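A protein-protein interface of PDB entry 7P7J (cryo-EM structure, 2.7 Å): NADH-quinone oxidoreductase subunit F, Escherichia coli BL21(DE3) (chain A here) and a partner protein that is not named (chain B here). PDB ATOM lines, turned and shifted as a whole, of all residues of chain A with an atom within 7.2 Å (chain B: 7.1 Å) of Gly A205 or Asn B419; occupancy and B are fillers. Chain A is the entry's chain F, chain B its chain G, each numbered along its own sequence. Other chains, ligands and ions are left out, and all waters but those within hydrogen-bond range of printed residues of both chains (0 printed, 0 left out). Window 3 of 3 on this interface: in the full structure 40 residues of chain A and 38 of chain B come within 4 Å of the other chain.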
ATOM      1  N   TYR A  83      21.471   2.187   1.758  1.00  0.00           N
ATOM      2  CA  TYR A  83      22.297   2.777   0.716  1.00  0.00           C
ATOM      3  C   TYR A  83      23.697   3.075   1.231  1.00  0.00           C
ATOM      4  O   TYR A  83      23.878   3.549   2.358  1.00  0.00           O
ATOM      5  CB  TYR A  83      21.664   4.058   0.174  1.00  0.00           C
ATOM      6  CG  TYR A  83      20.359   3.820  -0.544  1.00  0.00           C
ATOM      7  CD1 TYR A  83      20.341   3.404  -1.867  1.00  0.00           C
ATOM      8  CD2 TYR A  83      19.146   4.010   0.101  1.00  0.00           C
ATOM      9  CE1 TYR A  83      19.153   3.182  -2.526  1.00  0.00           C
ATOM     10  CE2 TYR A  83      17.953   3.792  -0.551  1.00  0.00           C
ATOM     11  CZ  TYR A  83      17.963   3.379  -1.863  1.00  0.00           C
ATOM     12  OH  TYR A  83      16.776   3.159  -2.518  1.00  0.00           O
ATOM     13  N   LEU A  85      27.064   5.210  -0.044  1.00  0.00           N
ATOM     14  CA  LEU A  85      27.507   6.230  -0.978  1.00  0.00           C
ATOM     15  C   LEU A  85      29.004   6.444  -0.828  1.00  0.00           C
ATOM     16  O   LEU A  85      29.532   6.465   0.288  1.00  0.00           O
ATOM     17  CB  LEU A  85      26.758   7.547  -0.756  1.00  0.00           C
ATOM     18  CG  LEU A  85      25.233   7.447  -0.678  1.00  0.00           C
ATOM     19  CD1 LEU A  85      24.608   8.823  -0.565  1.00  0.00           C
ATOM     20  CD2 LEU A  85      24.672   6.708  -1.876  1.00  0.00           C
ATOM     21  N   ILE A 184      23.868  13.634  -0.408  1.00  0.00           N
ATOM     22  CA  ILE A 184      22.607  12.901  -0.426  1.00  0.00           C
ATOM     23  C   ILE A 184      21.546  13.685  -1.185  1.00  0.00           C
ATOM     24  O   ILE A 184      20.789  13.122  -1.987  1.00  0.00           O
ATOM     25  CB  ILE A 184      22.173  12.586   1.016  1.00  0.00           C
ATOM     26  CG1 ILE A 184      23.094  11.529   1.618  1.00  0.00           C
ATOM     27  CG2 ILE A 184      20.735  12.126   1.070  1.00  0.00           C
ATOM     28  CD1 ILE A 184      22.834  11.265   3.066  1.00  0.00           C
ATOM     29  N   ASN A 185      21.485  15.000  -0.956  1.00  0.00           N
ATOM     30  CA  ASN A 185      20.515  15.841  -1.654  1.00  0.00           C
ATOM     31  C   ASN A 185      20.777  15.881  -3.156  1.00  0.00           C
ATOM     32  O   ASN A 185      19.836  15.840  -3.956  1.00  0.00           O
ATOM     33  CB  ASN A 185      20.531  17.252  -1.072  1.00  0.00           C
ATOM     34  CG  ASN A 185      19.412  17.484  -0.084  1.00  0.00           C
ATOM     35  OD1 ASN A 185      18.321  16.938  -0.228  1.00  0.00           O
ATOM     36  ND2 ASN A 185      19.674  18.301   0.927  1.00  0.00           N
ATOM     37  N   GLU A 188      19.665  12.720  -4.837  1.00  0.00           N
ATOM     38  CA  GLU A 188      18.225  12.730  -5.046  1.00  0.00           C
ATOM     39  C   GLU A 188      17.793  13.675  -6.159  1.00  0.00           C
ATOM     40  O   GLU A 188      16.591  13.841  -6.371  1.00  0.00           O
ATOM     41  CB  GLU A 188      17.507  13.115  -3.753  1.00  0.00           C
ATOM     42  CG  GLU A 188      17.681  12.136  -2.614  1.00  0.00           C
ATOM     43  CD  GLU A 188      16.926  12.563  -1.376  1.00  0.00           C
ATOM     44  OE1 GLU A 188      16.226  13.593  -1.436  1.00  0.00           O
ATOM     45  OE2 GLU A 188      17.033  11.878  -0.340  1.00  0.00           O
ATOM     46  N   ARG A 190      18.222  16.962  -6.284  1.00  0.00           N
ATOM     47  CA  ARG A 190      17.815  18.248  -5.745  1.00  0.00           C
ATOM     48  C   ARG A 190      18.999  19.208  -5.744  1.00  0.00           C
ATOM     49  O   ARG A 190      20.123  18.853  -6.107  1.00  0.00           O
ATOM     50  CB  ARG A 190      17.248  18.081  -4.336  1.00  0.00           C
ATOM     51  CG  ARG A 190      16.244  16.962  -4.208  1.00  0.00           C
ATOM     52  CD  ARG A 190      15.762  16.830  -2.781  1.00  0.00           C
ATOM     53  NE  ARG A 190      14.768  15.776  -2.639  1.00  0.00           N
ATOM     54  CZ  ARG A 190      13.466  15.948  -2.815  1.00  0.00           C
ATOM     55  NH1 ARG A 190      12.964  17.126  -3.147  1.00  0.00           N
ATOM     56  NH2 ARG A 190      12.648  14.912  -2.658  1.00  0.00           N
ATOM     57  N   ARG A 195      21.839  19.178   4.807  1.00  0.00           N
ATOM     58  CA  ARG A 195      20.781  18.988   5.784  1.00  0.00           C
ATOM     59  C   ARG A 195      21.314  19.189   7.196  1.00  0.00           C
ATOM     60  O   ARG A 195      22.523  19.206   7.436  1.00  0.00           O
ATOM     61  CB  ARG A 195      20.166  17.597   5.655  1.00  0.00           C
ATOM     62  CG  ARG A 195      19.605  17.301   4.285  1.00  0.00           C
ATOM     63  CD  ARG A 195      19.120  15.875   4.205  1.00  0.00           C
ATOM     64  NE  ARG A 195      18.668  15.535   2.863  1.00  0.00           N
ATOM     65  CZ  ARG A 195      18.306  14.318   2.486  1.00  0.00           C
ATOM     66  NH1 ARG A 195      18.332  13.298   3.326  1.00  0.00           N
ATOM     67  NH2 ARG A 195      17.911  14.119   1.234  1.00  0.00           N
ATOM     68  N   PRO A 199      18.253  14.513  12.460  1.00  0.00           N
ATOM     69  CA  PRO A 199      18.694  13.121  12.304  1.00  0.00           C
ATOM     70  C   PRO A 199      19.897  12.935  11.387  1.00  0.00           C
ATOM     71  O   PRO A 199      20.068  13.660  10.409  1.00  0.00           O
ATOM     72  CB  PRO A 199      17.464  12.441  11.707  1.00  0.00           C
ATOM     73  CG  PRO A 199      16.818  13.501  10.921  1.00  0.00           C
ATOM     74  CD  PRO A 199      17.028  14.777  11.687  1.00  0.00           C
ATOM     75  N   PHE A 200      20.719  11.953  11.721  1.00  0.00           N
ATOM     76  CA  PHE A 200      21.895  11.623  10.940  1.00  0.00           C
ATOM     77  C   PHE A 200      21.502  10.837   9.693  1.00  0.00           C
ATOM     78  O   PHE A 200      20.410  10.271   9.627  1.00  0.00           O
ATOM     79  CB  PHE A 200      22.874  10.829  11.798  1.00  0.00           C
ATOM     80  CG  PHE A 200      23.673  11.682  12.737  1.00  0.00           C
ATOM     81  CD1 PHE A 200      23.156  12.054  13.965  1.00  0.00           C
ATOM     82  CD2 PHE A 200      24.934  12.125  12.383  1.00  0.00           C
ATOM     83  CE1 PHE A 200      23.886  12.847  14.827  1.00  0.00           C
ATOM     84  CE2 PHE A 200      25.669  12.917  13.240  1.00  0.00           C
ATOM     85  CZ  PHE A 200      25.143  13.279  14.464  1.00  0.00           C
ATOM     86  N   PRO A 201      22.365  10.822   8.670  1.00  0.00           N
ATOM     87  CA  PRO A 201      22.085   9.988   7.489  1.00  0.00           C
ATOM     88  C   PRO A 201      21.973   8.504   7.787  1.00  0.00           C
ATOM     89  O   PRO A 201      21.314   7.785   7.025  1.00  0.00           O
ATOM     90  CB  PRO A 201      23.278  10.285   6.573  1.00  0.00           C
ATOM     91  CG  PRO A 201      23.667  11.665   6.927  1.00  0.00           C
ATOM     92  CD  PRO A 201      23.447  11.789   8.406  1.00  0.00           C
ATOM     93  N   ALA A 202      22.599   8.020   8.862  1.00  0.00           N
ATOM     94  CA  ALA A 202      22.451   6.619   9.242  1.00  0.00           C
ATOM     95  C   ALA A 202      21.022   6.296   9.654  1.00  0.00           C
ATOM     96  O   ALA A 202      20.540   5.188   9.401  1.00  0.00           O
ATOM     97  CB  ALA A 202      23.418   6.276  10.370  1.00  0.00           C
ATOM     98  N   THR A 203      20.331   7.245  10.285  1.00  0.00           N
ATOM     99  CA  THR A 203      18.933   7.039  10.645  1.00  0.00           C
ATOM    100  C   THR A 203      18.027   7.187   9.425  1.00  0.00           C
ATOM    101  O   THR A 203      17.191   6.317   9.156  1.00  0.00           O
ATOM    102  CB  THR A 203      18.536   8.021  11.753  1.00  0.00           C
ATOM    103  OG1 THR A 203      18.980   7.513  13.017  1.00  0.00           O
ATOM    104  CG2 THR A 203      17.029   8.220  11.810  1.00  0.00           C
ATOM    105  N   SER A 204      18.199   8.267   8.662  1.00  0.00           N
ATOM    106  CA  SER A 204      17.390   8.504   7.468  1.00  0.00           C
ATOM    107  C   SER A 204      18.206   9.389   6.530  1.00  0.00           C
ATOM    108  O   SER A 204      18.313  10.598   6.751  1.00  0.00           O
ATOM    109  CB  SER A 204      16.058   9.148   7.825  1.00  0.00           C
ATOM    110  OG  SER A 204      16.254  10.424   8.402  1.00  0.00           O
ATOM    111  N   GLY A 205      18.773   8.782   5.492  1.00  0.00           N
ATOM    112  CA  GLY A 205      19.609   9.507   4.558  1.00  0.00           C
ATOM    113  C   GLY A 205      19.018   9.626   3.170  1.00  0.00           C
ATOM    114  O   GLY A 205      18.150  10.469   2.931  1.00  0.00           O
ATOM    115  N   ALA A 206      19.484   8.790   2.247  1.00  0.00           N
ATOM    116  CA  ALA A 206      19.040   8.861   0.862  1.00  0.00           C
ATOM    117  C   ALA A 206      17.616   8.335   0.743  1.00  0.00           C
ATOM    118  O   ALA A 206      17.357   7.162   1.034  1.00  0.00           O
ATOM    119  CB  ALA A 206      19.983   8.068  -0.036  1.00  0.00           C
ATOM    120  N   TRP A 207      16.703   9.215   0.318  1.00  0.00           N
ATOM    121  CA  TRP A 207      15.277   8.918   0.167  1.00  0.00           C
ATOM    122  C   TRP A 207      14.664   8.413   1.472  1.00  0.00           C
ATOM    123  O   TRP A 207      13.808   7.528   1.476  1.00  0.00           O
ATOM    124  CB  TRP A 207      15.028   7.930  -0.974  1.00  0.00           C
ATOM    125  CG  TRP A 207      15.568   8.394  -2.285  1.00  0.00           C
ATOM    126  CD1 TRP A 207      15.043   9.358  -3.089  1.00  0.00           C
ATOM    127  CD2 TRP A 207      16.743   7.914  -2.945  1.00  0.00           C
ATOM    128  NE1 TRP A 207      15.818   9.511  -4.211  1.00  0.00           N
ATOM    129  CE2 TRP A 207      16.867   8.635  -4.146  1.00  0.00           C
ATOM    130  CE3 TRP A 207      17.701   6.946  -2.638  1.00  0.00           C
ATOM    131  CZ2 TRP A 207      17.912   8.419  -5.038  1.00  0.00           C
ATOM    132  CZ3 TRP A 207      18.735   6.733  -3.524  1.00  0.00           C
ATOM    133  CH2 TRP A 207      18.833   7.467  -4.710  1.00  0.00           C
ATOM    134  N   GLY A 208      15.113   8.976   2.591  1.00  0.00           N
ATOM    135  CA  GLY A 208      14.581   8.608   3.885  1.00  0.00           C
ATOM    136  C   GLY A 208      15.028   7.264   4.405  1.00  0.00           C
ATOM    137  O   GLY A 208      14.534   6.824   5.447  1.00  0.00           O
ATOM    138  N   LYS A 209      15.940   6.604   3.722  1.00  0.00           N
ATOM    139  CA  LYS A 209      16.428   5.289   4.086  1.00  0.00           C
ATOM    140  C   LYS A 209      17.751   5.402   4.823  1.00  0.00           C
ATOM    141  O   LYS A 209      18.440   6.420   4.725  1.00  0.00           O
ATOM    142  CB  LYS A 209      16.602   4.425   2.835  1.00  0.00           C
ATOM    143  CG  LYS A 209      15.362   4.346   1.967  1.00  0.00           C
ATOM    144  CD  LYS A 209      14.210   3.701   2.711  1.00  0.00           C
ATOM    145  CE  LYS A 209      12.969   3.629   1.839  1.00  0.00           C
ATOM    146  NZ  LYS A 209      12.516   4.980   1.408  1.00  0.00           N
ATOM    147  N   PRO A 210      18.111   4.392   5.616  1.00  0.00           N
ATOM    148  CA  PRO A 210      19.453   4.363   6.210  1.00  0.00           C
ATOM    149  C   PRO A 210      20.541   4.368   5.144  1.00  0.00           C
ATOM    150  O   PRO A 210      20.542   3.550   4.217  1.00  0.00           O
ATOM    151  CB  PRO A 210      19.460   3.065   7.028  1.00  0.00           C
ATOM    152  CG  PRO A 210      18.123   2.416   6.798  1.00  0.00           C
ATOM    153  CD  PRO A 210      17.200   3.450   6.281  1.00  0.00           C
ATOM    154  N   THR A 211      21.466   5.311   5.285  1.00  0.00           N
ATOM    155  CA  THR A 211      22.449   5.605   4.255  1.00  0.00           C
ATOM    156  C   THR A 211      23.759   5.970   4.931  1.00  0.00           C
ATOM    157  O   THR A 211      23.771   6.782   5.858  1.00  0.00           O
ATOM    158  CB  THR A 211      21.971   6.755   3.364  1.00  0.00           C
ATOM    159  OG1 THR A 211      20.734   6.394   2.740  1.00  0.00           O
ATOM    160  CG2 THR A 211      22.991   7.069   2.295  1.00  0.00           C
ATOM    161  N   CYS A 212      24.851   5.370   4.472  1.00  0.00           N
ATOM    162  CA  CYS A 212      26.177   5.693   4.983  1.00  0.00           C
ATOM    163  C   CYS A 212      27.043   6.227   3.854  1.00  0.00           C
ATOM    164  O   CYS A 212      27.165   5.587   2.807  1.00  0.00           O
ATOM    165  CB  CYS A 212      26.836   4.478   5.635  1.00  0.00           C
ATOM    166  SG  CYS A 212      26.637   4.412   7.428  1.00  0.00           S
ATOM    167  N   ALA B 400       3.353  11.617   6.514  1.00  0.00           N
ATOM    168  CA  ALA B 400       4.776  11.898   6.674  1.00  0.00           C
ATOM    169  C   ALA B 400       5.069  12.411   8.074  1.00  0.00           C
ATOM    170  O   ALA B 400       6.105  12.073   8.664  1.00  0.00           O
ATOM    171  CB  ALA B 400       5.232  12.908   5.625  1.00  0.00           C
ATOM    172  N   GLN B 413      10.782  20.140  13.013  1.00  0.00           N
ATOM    173  CA  GLN B 413      11.906  19.925  12.104  1.00  0.00           C
ATOM    174  C   GLN B 413      11.348  19.419  10.779  1.00  0.00           C
ATOM    175  O   GLN B 413      11.347  18.227  10.477  1.00  0.00           O
ATOM    176  CB  GLN B 413      12.913  18.957  12.710  1.00  0.00           C
ATOM    177  CG  GLN B 413      14.262  18.969  12.016  1.00  0.00           C
ATOM    178  CD  GLN B 413      15.356  18.360  12.863  1.00  0.00           C
ATOM    179  OE1 GLN B 413      15.107  17.878  13.967  1.00  0.00           O
ATOM    180  NE2 GLN B 413      16.581  18.384  12.352  1.00  0.00           N
ATOM    181  N   ILE B 414      10.879  20.372   9.971  1.00  0.00           N
ATOM    182  CA  ILE B 414      10.069  20.061   8.797  1.00  0.00           C
ATOM    183  C   ILE B 414      10.888  19.360   7.712  1.00  0.00           C
ATOM    184  O   ILE B 414      10.364  18.494   6.998  1.00  0.00           O
ATOM    185  CB  ILE B 414       9.395  21.355   8.292  1.00  0.00           C
ATOM    186  CG1 ILE B 414       8.542  21.098   7.048  1.00  0.00           C
ATOM    187  CG2 ILE B 414      10.420  22.456   8.061  1.00  0.00           C
ATOM    188  CD1 ILE B 414       7.410  20.132   7.287  1.00  0.00           C
ATOM    189  N   ALA B 415      12.175  19.700   7.578  1.00  0.00           N
ATOM    190  CA  ALA B 415      13.008  19.091   6.545  1.00  0.00           C
ATOM    191  C   ALA B 415      13.189  17.597   6.777  1.00  0.00           C
ATOM    192  O   ALA B 415      13.113  16.803   5.834  1.00  0.00           O
ATOM    193  CB  ALA B 415      14.363  19.791   6.484  1.00  0.00           C
ATOM    194  N   ALA B 416      13.401  17.196   8.032  1.00  0.00           N
ATOM    195  CA  ALA B 416      13.510  15.778   8.354  1.00  0.00           C
ATOM    196  C   ALA B 416      12.185  15.055   8.150  1.00  0.00           C
ATOM    197  O   ALA B 416      12.167  13.888   7.742  1.00  0.00           O
ATOM    198  CB  ALA B 416      13.994  15.607   9.789  1.00  0.00           C
ATOM    199  N   ILE B 417      11.069  15.730   8.443  1.00  0.00           N
ATOM    200  CA  ILE B 417       9.748  15.140   8.234  1.00  0.00           C
ATOM    201  C   ILE B 417       9.513  14.873   6.755  1.00  0.00           C
ATOM    202  O   ILE B 417       9.028  13.803   6.370  1.00  0.00           O
ATOM    203  CB  ILE B 417       8.656  16.052   8.823  1.00  0.00           C
ATOM    204  CG1 ILE B 417       8.834  16.200  10.331  1.00  0.00           C
ATOM    205  CG2 ILE B 417       7.275  15.506   8.516  1.00  0.00           C
ATOM    206  CD1 ILE B 417       7.869  17.165  10.959  1.00  0.00           C
ATOM    207  N   LEU B 418       9.863  15.837   5.903  1.00  0.00           N
ATOM    208  CA  LEU B 418       9.694  15.641   4.467  1.00  0.00           C
ATOM    209  C   LEU B 418      10.694  14.633   3.915  1.00  0.00           C
ATOM    210  O   LEU B 418      10.399  13.958   2.923  1.00  0.00           O
ATOM    211  CB  LEU B 418       9.823  16.976   3.736  1.00  0.00           C
ATOM    212  CG  LEU B 418       8.812  18.049   4.140  1.00  0.00           C
ATOM    213  CD1 LEU B 418       9.041  19.330   3.356  1.00  0.00           C
ATOM    214  CD2 LEU B 418       7.393  17.548   3.955  1.00  0.00           C
ATOM    215  N   ASN B 419      11.873  14.525   4.528  1.00  0.00           N
ATOM    216  CA  ASN B 419      12.849  13.535   4.084  1.00  0.00           C
ATOM    217  C   ASN B 419      12.386  12.119   4.404  1.00  0.00           C
ATOM    218  O   ASN B 419      12.491  11.219   3.564  1.00  0.00           O
ATOM    219  CB  ASN B 419      14.207  13.811   4.728  1.00  0.00           C
ATOM    220  CG  ASN B 419      15.239  12.760   4.379  1.00  0.00           C
ATOM    221  OD1 ASN B 419      15.386  12.380   3.219  1.00  0.00           O
ATOM    222  ND2 ASN B 419      15.956  12.277   5.385  1.00  0.00           N
ATOM    223  N   ILE B 420      11.884  11.901   5.622  1.00  0.00           N
ATOM    224  CA  ILE B 420      11.409  10.574   6.005  1.00  0.00           C
ATOM    225  C   ILE B 420      10.164  10.202   5.207  1.00  0.00           C
ATOM    226  O   ILE B 420      10.077   9.113   4.628  1.00  0.00           O
ATOM    227  CB  ILE B 420      11.151  10.518   7.520  1.00  0.00           C
ATOM    228  CG1 ILE B 420      12.469  10.657   8.283  1.00  0.00           C
ATOM    229  CG2 ILE B 420      10.454   9.227   7.903  1.00  0.00           C
ATOM    230  CD1 ILE B 420      12.296  10.811   9.772  1.00  0.00           C
ATOM    231  N   GLY B 421       9.191  11.103   5.156  1.00  0.00           N
ATOM    232  CA  GLY B 421       8.031  10.929   4.309  1.00  0.00           C
ATOM    233  C   GLY B 421       8.269  11.417   2.896  1.00  0.00           C
ATOM    234  O   GLY B 421       7.846  12.524   2.547  1.00  0.00           O
ATOM    235  N   GLN B 422       8.968  10.619   2.089  1.00  0.00           N
ATOM    236  CA  GLN B 422       9.350  11.001   0.733  1.00  0.00           C
ATOM    237  C   GLN B 422       8.146  11.280  -0.156  1.00  0.00           C
ATOM    238  O   GLN B 422       7.926  12.418  -0.579  1.00  0.00           O
ATOM    239  CB  GLN B 422      10.203   9.901   0.103  1.00  0.00           C
ATOM    240  CG  GLN B 422      11.611   9.851   0.628  1.00  0.00           C
ATOM    241  CD  GLN B 422      12.428  11.039   0.184  1.00  0.00           C
ATOM    242  OE1 GLN B 422      12.395  11.428  -0.981  1.00  0.00           O
ATOM    243  NE2 GLN B 422      13.168  11.628   1.114  1.00  0.00           N
ATOM    244  N   ARG B 423       7.362  10.246  -0.439  1.00  0.00           N
ATOM    245  CA  ARG B 423       6.130  10.397  -1.189  1.00  0.00           C
ATOM    246  C   ARG B 423       4.971   9.675  -0.528  1.00  0.00           C
ATOM    247  O   ARG B 423       3.865   9.680  -1.078  1.00  0.00           O
ATOM    248  CB  ARG B 423       6.301   9.888  -2.628  1.00  0.00           C
ATOM    249  CG  ARG B 423       6.919  10.903  -3.570  1.00  0.00           C
ATOM    250  CD  ARG B 423       6.931  10.394  -4.999  1.00  0.00           C
ATOM    251  NE  ARG B 423       7.728  11.247  -5.872  1.00  0.00           N
ATOM    252  CZ  ARG B 423       8.211  10.873  -7.049  1.00  0.00           C
ATOM    253  NH1 ARG B 423       7.997   9.660  -7.531  1.00  0.00           N
ATOM    254  NH2 ARG B 423       8.928  11.739  -7.761  1.00  0.00           N
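Printed residues of chain A that touch a printed residue of chain B: Glu A188, Arg A190, Arg A195, Pro A199, Ser A204, Gly A205, Trp A207 and Gly A208.
Hydrophobic or aromatic side chains of chain A that line the printed part of chain B: Pro A199 and Trp A207.
Among the printed residues, no Asp or Glu carboxylate lies within 4 Å of a Lys or Arg side-chain nitrogen of the other chain.
The side-chain carboxylate (OE1) of Glu A188 is in salt-bridge range of the guanidinium group (NE) of Arg A190 (2.9 Å).
The side-chain carboxylate (OE2) of Glu A188 lies within salt-bridge range of the guanidinium group (NH2) of Arg A195, at 2.9 Å.
The side-chain carboxylate (OE2) of Glu A188 lies within hydrogen-bond range of the backbone NH (N) of Trp A207 (2.8 Å).
The backbone carbonyl oxygen (O) of Gly A205 sits at hydrogen-bond distance from the guanidinium group (NH1) of Arg A195 (2.9 Å).
The backbone carbonyl oxygen (O) of Trp A207 sits at hydrogen-bond distance from the side-chain amino group (NZ) of Lys A209 (2.9 Å).
The side-chain amide nitrogen (NE2) of Gln B422 lies within hydrogen-bond range of the backbone carbonyl oxygen (O) of Asn B419.
The guanidinium group (NH1) of Arg A195 lies within hydrogen-bond range of the side-chain amide oxygen (OD1) of Asn B419 (3.1 Å).
The backbone carbonyl oxygen (O) of Ser A204 is in hydrogen-bond range of the side-chain amide nitrogen (ND2) of Asn B419, at 3.2 Å.
The backbone carbonyl oxygen (O) of Gly A205 sits close to the side-chain amide oxygen (OD1) of Asn B419 (3.4 Å).
The backbone NH (N) of Gly A208 sits at hydrogen-bond distance from the side-chain amide oxygen (OD1) of Asn B419 (3.5 Å).
Among the printed residues, pairs that only touch across the chains: Trp A207 with Gln B422 (3.3 Å), Gly A208 with Gln B422 (3.6 Å), Pro A199 with Ala B416 (3.7 Å), Pro A199 with Gln B413 (3.7 Å), Ser A204 with Ile B420 (3.8 Å), Arg A190 with Gln B422 (3.9 Å) and Glu A188 with Asn B419 (3.95 Å).
Gly A205 touches one residue of chain B.
Of chain A, only Glu A188, Arg A195, Ser A204, Gly A205 and Gly A208 come within 4 Å of Asn B419.
Printed residues of chain B within 4 Å of Trp A207: Gln B422 (3.3 Å).
Printed residues of chain A within 4 Å of Ala B416: Pro A199 (3.7 Å).
Of the printed residues of chain A, Ile B420 touches Ser A204.
Of the printed residues of chain A, Gln B422 touches Arg A190 (3.9 Å), Trp A207 (3.3 Å) and Gly A208 (3.6 Å).
Asn A185 touches none of the printed residues of chain B.
The nearest residue of chain A that does not touch Asn B419 is Trp A207 (4.1 Å).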
